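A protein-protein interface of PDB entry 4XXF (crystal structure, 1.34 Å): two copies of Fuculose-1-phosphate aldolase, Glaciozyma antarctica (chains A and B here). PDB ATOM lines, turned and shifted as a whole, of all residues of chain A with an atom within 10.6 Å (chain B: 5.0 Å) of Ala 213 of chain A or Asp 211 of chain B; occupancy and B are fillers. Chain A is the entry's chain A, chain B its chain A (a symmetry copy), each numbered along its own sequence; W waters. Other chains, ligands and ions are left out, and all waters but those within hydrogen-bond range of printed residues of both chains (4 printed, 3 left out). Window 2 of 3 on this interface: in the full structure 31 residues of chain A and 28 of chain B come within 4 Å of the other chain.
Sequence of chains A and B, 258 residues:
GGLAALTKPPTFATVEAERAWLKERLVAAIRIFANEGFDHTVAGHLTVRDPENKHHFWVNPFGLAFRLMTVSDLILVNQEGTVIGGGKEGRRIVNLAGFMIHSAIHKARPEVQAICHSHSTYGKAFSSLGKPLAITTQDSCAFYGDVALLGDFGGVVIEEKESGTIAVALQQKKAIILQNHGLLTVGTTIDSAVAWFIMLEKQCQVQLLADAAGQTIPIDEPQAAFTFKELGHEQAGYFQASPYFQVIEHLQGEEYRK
Ala 213 of chain A touches just these residues of chain B: Leu 208 and Asp 211. Asp 211 of chain B touches one residue of chain A. Printed residues of chain A within 4 Å of Ala 212 of chain B: Ala 212 (3.4 Å). No residue of chain A comes within 4 Å of Ala 213 of chain B. Gly 214 of chain B touches none of the printed residues of chain A. Of the printed residues of chain B, Ala 212 of chain A touches Ala 212 (3.4 Å). Of the printed residues of chain A, Leu 129 of chain B touches Ala 210 (3.7 Å), Gly 214 (3.8 Å), Gln 215 (3.6 Å), Thr 216 (3.9 Å) and Ile 217 (3.8 Å). Of the printed residues of chain B, Leu 209 of chain A touches Leu 208. Gln 205 of chain A touches none of the printed residues of chain B. Leu 209 of chain B touches none of the printed residues of chain A. The nearest residue of chain B that does not touch Ala 213 of chain A is Ala 212 of chain B (4.04 Å).
Leu 209 of chain A touches Leu 208 of chain B, but with the chains exchanged Leu 208 of chain A does not touch Leu 209 of chain B (9.0 Å). Ala 212 of chain A touches its own counterpart, Ala 212 of chain B. Ala 213 of chain A touches Leu 208 of chain B, but with the chains exchanged Leu 208 of chain A does not touch Ala 213 of chain B (10.0 Å). Ala 213 of chain A touches Asp 211 of chain B, but with the chains exchanged Asp 211 of chain A does not touch Ala 213 of chain B (9.2 Å). Of the 9 pairs that touch across the chains among the printed residues, 1 has its exchanged pair printed and touching as well.
OD2 of Asp 211 of chain B lies within hydrogen-bond range of NE2 of Gln 207 of chain B (3.1 Å).
Among the printed residues, pairs that only touch across the chains: Ala 212 of chain A with Ala 212 of chain B, Gln 215 of chain A with Leu 129 of chain B, Ala 213 of chain A with Leu 208 of chain B, Ala 210 of chain A with Leu 129 of chain B, Ile 217 of chain A with Leu 129 of chain B, Ala 213 of chain A with Asp 211 of chain B, Gly 214 of chain A with Leu 129 of chain B, Thr 216 of chain A with Leu 129 of chain B and Leu 209 of chain A with Leu 208 of chain B.
Water W2 bridges O of Gln 215 of chain A and O of Leu 129 of chain B. Water W3 lies within hydrogen-bond range of NZ of Lys 131 of chain B (2.6 Å), OD2 of Asp 211 of chain B (2.7 Å) and O of Ala 213 of chain A (2.8 Å). Water W1 lies within hydrogen-bond range of O of Leu 209 of chain A and O of Leu 208 of chain B. Water W4 bridges the backbone NH of Gln 215 of chain A (2.9 Å) and the side-chain amino group of Lys 131 of chain B (3.1 Å).
Hydrophobic or aromatic side chains of chain B within 4 Å of the printed part of chain A: Leu 129, Leu 208 and Ala 212. Of the 13 printed residues of chain A, 8 touch a printed residue of chain B. Hydrophobic or aromatic side chains of chain A within 4 Å of the printed part of chain B: Ala 212, Ala 213 and Ile 217. Among the printed residues, 9 pairs touch across the chains. Among the printed residues, no Asp or Glu carboxylate lies within 4 Å of a Lys or Arg side-chain nitrogen of the other chain.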
ATOM      1  N   GLN A 205     -17.974  10.182  -7.056  1.00  0.00           N
ATOM      2  CA  GLN A 205     -16.921  10.436  -6.086  1.00  0.00           C
ATOM      3  C   GLN A 205     -17.441  11.233  -4.899  1.00  0.00           C
ATOM      4  O   GLN A 205     -17.167  10.904  -3.738  1.00  0.00           O
ATOM      5  CB  GLN A 205     -15.768  11.179  -6.756  1.00  0.00           C
ATOM      6  CG  GLN A 205     -14.565  11.414  -5.841  1.00  0.00           C
ATOM      7  CD  GLN A 205     -13.515  12.274  -6.496  1.00  0.00           C
ATOM      8  OE1 GLN A 205     -13.705  12.770  -7.613  1.00  0.00           O
ATOM      9  NE2 GLN A 205     -12.382  12.443  -5.818  1.00  0.00           N
ATOM     10  N   VAL A 206     -18.197  12.283  -5.201  1.00  0.00           N
ATOM     11  CA  VAL A 206     -18.781  13.150  -4.189  1.00  0.00           C
ATOM     12  C   VAL A 206     -19.747  12.371  -3.290  1.00  0.00           C
ATOM     13  O   VAL A 206     -19.706  12.508  -2.064  1.00  0.00           O
ATOM     14  CB  VAL A 206     -19.497  14.347  -4.856  1.00  0.00           C
ATOM     15  CG1 VAL A 206     -20.434  15.030  -3.888  1.00  0.00           C
ATOM     16  CG2 VAL A 206     -18.463  15.330  -5.415  1.00  0.00           C
ATOM     17  N   GLN A 207     -20.600  11.543  -3.877  1.00  0.00           N
ATOM     18  CA  GLN A 207     -21.550  10.790  -3.071  1.00  0.00           C
ATOM     19  C   GLN A 207     -20.836   9.783  -2.165  1.00  0.00           C
ATOM     20  O   GLN A 207     -21.230   9.618  -1.012  1.00  0.00           O
ATOM     21  CB  GLN A 207     -22.589  10.066  -3.938  1.00  0.00           C
ATOM     22  CG  GLN A 207     -23.588   9.267  -3.072  1.00  0.00           C
ATOM     23  CD  GLN A 207     -24.942   9.035  -3.704  1.00  0.00           C
ATOM     24  OE1 GLN A 207     -25.230   9.481  -4.825  1.00  0.00           O
ATOM     25  NE2 GLN A 207     -25.784   8.315  -2.983  1.00  0.00           N
ATOM     26  N   LEU A 208     -19.798   9.114  -2.673  1.00  0.00           N
ATOM     27  CA  LEU A 208     -19.038   8.168  -1.842  1.00  0.00           C
ATOM     28  C   LEU A 208     -18.392   8.890  -0.650  1.00  0.00           C
ATOM     29  O   LEU A 208     -18.397   8.385   0.474  1.00  0.00           O
ATOM     30  CB  LEU A 208     -17.975   7.441  -2.676  1.00  0.00           C
ATOM     31  CG  LEU A 208     -18.541   6.471  -3.716  1.00  0.00           C
ATOM     32  CD1 LEU A 208     -17.496   6.133  -4.770  1.00  0.00           C
ATOM     33  CD2 LEU A 208     -19.085   5.207  -3.047  1.00  0.00           C
ATOM     34  N   LEU A 209     -17.846  10.079  -0.893  1.00  0.00           N
ATOM     35  CA  LEU A 209     -17.246  10.898   0.175  1.00  0.00           C
ATOM     36  C   LEU A 209     -18.275  11.313   1.220  1.00  0.00           C
ATOM     37  O   LEU A 209     -18.081  11.150   2.421  1.00  0.00           O
ATOM     38  CB  LEU A 209     -16.605  12.157  -0.405  1.00  0.00           C
ATOM     39  CG  LEU A 209     -15.263  11.982  -1.118  1.00  0.00           C
ATOM     40  CD1 LEU A 209     -14.976  13.181  -2.011  1.00  0.00           C
ATOM     41  CD2 LEU A 209     -14.141  11.797  -0.092  1.00  0.00           C
ATOM     42  N   ALA A 210     -19.388  11.861   0.751  1.00  0.00           N
ATOM     43  CA  ALA A 210     -20.391  12.413   1.642  1.00  0.00           C
ATOM     44  C   ALA A 210     -21.136  11.317   2.404  1.00  0.00           C
ATOM     45  O   ALA A 210     -21.368  11.449   3.609  1.00  0.00           O
ATOM     46  CB  ALA A 210     -21.371  13.289   0.854  1.00  0.00           C
ATOM     47  N   ASP A 211     -21.505  10.236   1.720  1.00  0.00           N
ATOM     48  CA  ASP A 211     -22.261   9.174   2.376  1.00  0.00           C
ATOM     49  C   ASP A 211     -21.418   8.483   3.440  1.00  0.00           C
ATOM     50  O   ASP A 211     -21.953   8.032   4.455  1.00  0.00           O
ATOM     51  CB  ASP A 211     -22.770   8.144   1.362  1.00  0.00           C
ATOM     52  CG  ASP A 211     -24.003   8.608   0.587  1.00  0.00           C
ATOM     53  OD1 ASP A 211     -24.455   9.765   0.734  1.00  0.00           O
ATOM     54  OD2 ASP A 211     -24.523   7.792  -0.205  1.00  0.00           O
ATOM     55  N   ALA A 212     -20.106   8.391   3.223  1.00  0.00           N
ATOM     56  CA  ALA A 212     -19.247   7.800   4.251  1.00  0.00           C
ATOM     57  C   ALA A 212     -19.178   8.693   5.485  1.00  0.00           C
ATOM     58  O   ALA A 212     -19.031   8.201   6.593  1.00  0.00           O
ATOM     59  CB  ALA A 212     -17.845   7.550   3.712  1.00  0.00           C
ATOM     60  N   ALA A 213     -19.271  10.006   5.280  1.00  0.00           N
ATOM     61  CA  ALA A 213     -19.082  10.974   6.360  1.00  0.00           C
ATOM     62  C   ALA A 213     -20.349  11.309   7.136  1.00  0.00           C
ATOM     63  O   ALA A 213     -20.275  11.677   8.314  1.00  0.00           O
ATOM     64  CB  ALA A 213     -18.474  12.253   5.795  1.00  0.00           C
ATOM     65  N   GLY A 214     -21.513  11.216   6.504  1.00  0.00           N
ATOM     66  CA  GLY A 214     -22.727  11.648   7.169  1.00  0.00           C
ATOM     67  C   GLY A 214     -23.947  11.511   6.292  1.00  0.00           C
ATOM     68  O   GLY A 214     -23.965  10.744   5.328  1.00  0.00           O
ATOM     69  N   GLN A 215     -24.972  12.287   6.620  1.00  0.00           N
ATOM     70  CA  GLN A 215     -26.240  12.244   5.909  1.00  0.00           C
ATOM     71  C   GLN A 215     -26.387  13.431   4.962  1.00  0.00           C
ATOM     72  O   GLN A 215     -26.425  14.580   5.405  1.00  0.00           O
ATOM     73  CB  GLN A 215     -27.399  12.223   6.913  1.00  0.00           C
ATOM     74  CG  GLN A 215     -28.773  12.256   6.267  1.00  0.00           C
ATOM     75  CD  GLN A 215     -29.014  11.063   5.365  1.00  0.00           C
ATOM     76  OE1 GLN A 215     -28.977   9.916   5.813  1.00  0.00           O
ATOM     77  NE2 GLN A 215     -29.246  11.326   4.083  1.00  0.00           N
ATOM     78  N   THR A 216     -26.468  13.166   3.664  1.00  0.00           N
ATOM     79  CA  THR A 216     -26.661  14.251   2.717  1.00  0.00           C
ATOM     80  C   THR A 216     -28.068  14.840   2.784  1.00  0.00           C
ATOM     81  O   THR A 216     -29.022  14.196   3.224  1.00  0.00           O
ATOM     82  CB  THR A 216     -26.390  13.804   1.270  1.00  0.00           C
ATOM     83  OG1 THR A 216     -27.224  12.686   0.953  1.00  0.00           O
ATOM     84  CG2 THR A 216     -24.933  13.414   1.085  1.00  0.00           C
ATOM     85  N   ILE A 217     -28.169  16.082   2.329  1.00  0.00           N
ATOM     86  CA  ILE A 217     -29.444  16.761   2.169  1.00  0.00           C
ATOM     87  C   ILE A 217     -29.701  16.916   0.677  1.00  0.00           C
ATOM     88  O   ILE A 217     -28.924  17.576  -0.015  1.00  0.00           O
ATOM     89  CB  ILE A 217     -29.437  18.141   2.854  1.00  0.00           C
ATOM     90  CG1 ILE A 217     -29.064  17.995   4.336  1.00  0.00           C
ATOM     91  CG2 ILE A 217     -30.787  18.822   2.688  1.00  0.00           C
ATOM     92  CD1 ILE A 217     -28.957  19.305   5.082  1.00  0.00           C
ATOM     93  N   LEU B 129     -23.766  18.075   3.100  1.00  0.00           N
ATOM     94  CA  LEU B 129     -24.183  17.611   4.425  1.00  0.00           C
ATOM     95  C   LEU B 129     -24.904  18.688   5.236  1.00  0.00           C
ATOM     96  O   LEU B 129     -25.513  18.385   6.252  1.00  0.00           O
ATOM     97  CB  LEU B 129     -22.959  17.116   5.212  1.00  0.00           C
ATOM     98  CG  LEU B 129     -22.153  15.981   4.584  1.00  0.00           C
ATOM     99  CD1 LEU B 129     -20.911  15.734   5.431  1.00  0.00           C
ATOM    100  CD2 LEU B 129     -22.981  14.715   4.451  1.00  0.00           C
ATOM    101  N   LYS B 131     -23.767  20.992   7.194  1.00  0.00           N
ATOM    102  CA  LYS B 131     -23.167  21.104   8.519  1.00  0.00           C
ATOM    103  C   LYS B 131     -22.173  22.256   8.558  1.00  0.00           C
ATOM    104  O   LYS B 131     -21.510  22.533   7.562  1.00  0.00           O
ATOM    105  CB  LYS B 131     -22.423  19.816   8.878  1.00  0.00           C
ATOM    106  CG  LYS B 131     -23.277  18.588   9.031  1.00  0.00           C
ATOM    107  CD  LYS B 131     -22.377  17.407   9.362  1.00  0.00           C
ATOM    108  CE  LYS B 131     -23.189  16.169   9.670  1.00  0.00           C
ATOM    109  NZ  LYS B 131     -22.301  15.054  10.099  1.00  0.00           N
ATOM    110  N   VAL B 206     -10.356  17.145   5.213  1.00  0.00           N
ATOM    111  CA  VAL B 206     -10.002  16.590   6.511  1.00  0.00           C
ATOM    112  C   VAL B 206     -11.252  16.142   7.276  1.00  0.00           C
ATOM    113  O   VAL B 206     -11.277  15.047   7.844  1.00  0.00           O
ATOM    114  CB  VAL B 206      -9.198  17.623   7.333  1.00  0.00           C
ATOM    115  CG1 VAL B 206      -9.162  17.247   8.796  1.00  0.00           C
ATOM    116  CG2 VAL B 206      -7.782  17.759   6.761  1.00  0.00           C
ATOM    117  N   GLN B 207     -12.295  16.961   7.282  1.00  0.00           N
ATOM    118  CA  GLN B 207     -13.503  16.591   8.007  1.00  0.00           C
ATOM    119  C   GLN B 207     -14.174  15.365   7.380  1.00  0.00           C
ATOM    120  O   GLN B 207     -14.655  14.498   8.107  1.00  0.00           O
ATOM    121  CB  GLN B 207     -14.503  17.752   8.084  1.00  0.00           C
ATOM    122  CG  GLN B 207     -15.781  17.346   8.850  1.00  0.00           C
ATOM    123  CD  GLN B 207     -16.528  18.487   9.503  1.00  0.00           C
ATOM    124  OE1 GLN B 207     -16.122  19.657   9.445  1.00  0.00           O
ATOM    125  NE2 GLN B 207     -17.646  18.148  10.123  1.00  0.00           N
ATOM    126  N   LEU B 208     -14.212  15.289   6.048  1.00  0.00           N
ATOM    127  CA  LEU B 208     -14.798  14.117   5.381  1.00  0.00           C
ATOM    128  C   LEU B 208     -14.025  12.841   5.746  1.00  0.00           C
ATOM    129  O   LEU B 208     -14.619  11.793   6.003  1.00  0.00           O
ATOM    130  CB  LEU B 208     -14.832  14.313   3.859  1.00  0.00           C
ATOM    131  CG  LEU B 208     -15.805  15.393   3.382  1.00  0.00           C
ATOM    132  CD1 LEU B 208     -15.476  15.832   1.962  1.00  0.00           C
ATOM    133  CD2 LEU B 208     -17.254  14.913   3.494  1.00  0.00           C
ATOM    134  N   LEU B 209     -12.698  12.934   5.783  1.00  0.00           N
ATOM    135  CA  LEU B 209     -11.844  11.798   6.175  1.00  0.00           C
ATOM    136  C   LEU B 209     -12.096  11.368   7.615  1.00  0.00           C
ATOM    137  O   LEU B 209     -12.309  10.196   7.914  1.00  0.00           O
ATOM    138  CB  LEU B 209     -10.367  12.155   6.026  1.00  0.00           C
ATOM    139  CG  LEU B 209      -9.804  12.176   4.604  1.00  0.00           C
ATOM    140  CD1 LEU B 209      -8.501  12.963   4.560  1.00  0.00           C
ATOM    141  CD2 LEU B 209      -9.582  10.745   4.103  1.00  0.00           C
ATOM    142  N   ALA B 210     -12.070  12.335   8.523  1.00  0.00           N
ATOM    143  CA  ALA B 210     -12.170  12.043   9.941  1.00  0.00           C
ATOM    144  C   ALA B 210     -13.577  11.587  10.326  1.00  0.00           C
ATOM    145  O   ALA B 210     -13.729  10.631  11.092  1.00  0.00           O
ATOM    146  CB  ALA B 210     -11.753  13.268  10.760  1.00  0.00           C
ATOM    147  N   ASP B 211     -14.604  12.251   9.801  1.00  0.00           N
ATOM    148  CA  ASP B 211     -15.972  11.897  10.165  1.00  0.00           C
ATOM    149  C   ASP B 211     -16.328  10.506   9.658  1.00  0.00           C
ATOM    150  O   ASP B 211     -17.106   9.795  10.297  1.00  0.00           O
ATOM    151  CB  ASP B 211     -16.976  12.923   9.627  1.00  0.00           C
ATOM    152  CG  ASP B 211     -17.038  14.208  10.453  1.00  0.00           C
ATOM    153  OD1 ASP B 211     -16.253  14.394  11.409  1.00  0.00           O
ATOM    154  OD2 ASP B 211     -17.888  15.062  10.121  1.00  0.00           O
ATOM    155  N   ALA B 212     -15.772  10.106   8.514  1.00  0.00           N
ATOM    156  CA  ALA B 212     -16.028   8.750   8.025  1.00  0.00           C
ATOM    157  C   ALA B 212     -15.377   7.711   8.931  1.00  0.00           C
ATOM    158  O   ALA B 212     -15.888   6.610   9.070  1.00  0.00           O
ATOM    159  CB  ALA B 212     -15.525   8.582   6.598  1.00  0.00           C
ATOM    160  N   ALA B 213     -14.244   8.067   9.533  1.00  0.00           N
ATOM    161  CA  ALA B 213     -13.452   7.118  10.316  1.00  0.00           C
ATOM    162  C   ALA B 213     -13.848   7.024  11.784  1.00  0.00           C
ATOM    163  O   ALA B 213     -13.649   5.980  12.414  1.00  0.00           O
ATOM    164  CB  ALA B 213     -11.974   7.479  10.207  1.00  0.00           C
ATOM    165  N   GLY B 214     -14.386   8.096  12.355  1.00  0.00           N
ATOM    166  CA  GLY B 214     -14.658   8.087  13.780  1.00  0.00           C
ATOM    167  C   GLY B 214     -15.227   9.397  14.268  1.00  0.00           C
ATOM    168  O   GLY B 214     -15.779  10.186  13.500  1.00  0.00           O
ATOM    169  N   THR B 216     -14.596  13.023  15.834  1.00  0.00           N
ATOM    170  CA  THR B 216     -13.610  14.060  16.081  1.00  0.00           C
ATOM    171  C   THR B 216     -13.755  14.686  17.466  1.00  0.00           C
ATOM    172  O   THR B 216     -14.820  14.653  18.085  1.00  0.00           O
ATOM    173  CB  THR B 216     -13.683  15.183  15.031  1.00  0.00           C
ATOM    174  OG1 THR B 216     -15.007  15.724  15.005  1.00  0.00           O
ATOM    175  CG2 THR B 216     -13.325  14.660  13.649  1.00  0.00           C
HETATM  176  O   HOH W   1     -15.555  10.592   3.530  1.00  0.00           O
HETATM  177  O   HOH W   2     -26.500  16.244   7.461  1.00  0.00           O
HETATM  178  O   HOH W   3     -20.103  14.464   8.742  1.00  0.00           O
HETATM  179  O   HOH W   4     -24.792  13.457   9.252  1.00  0.00           O
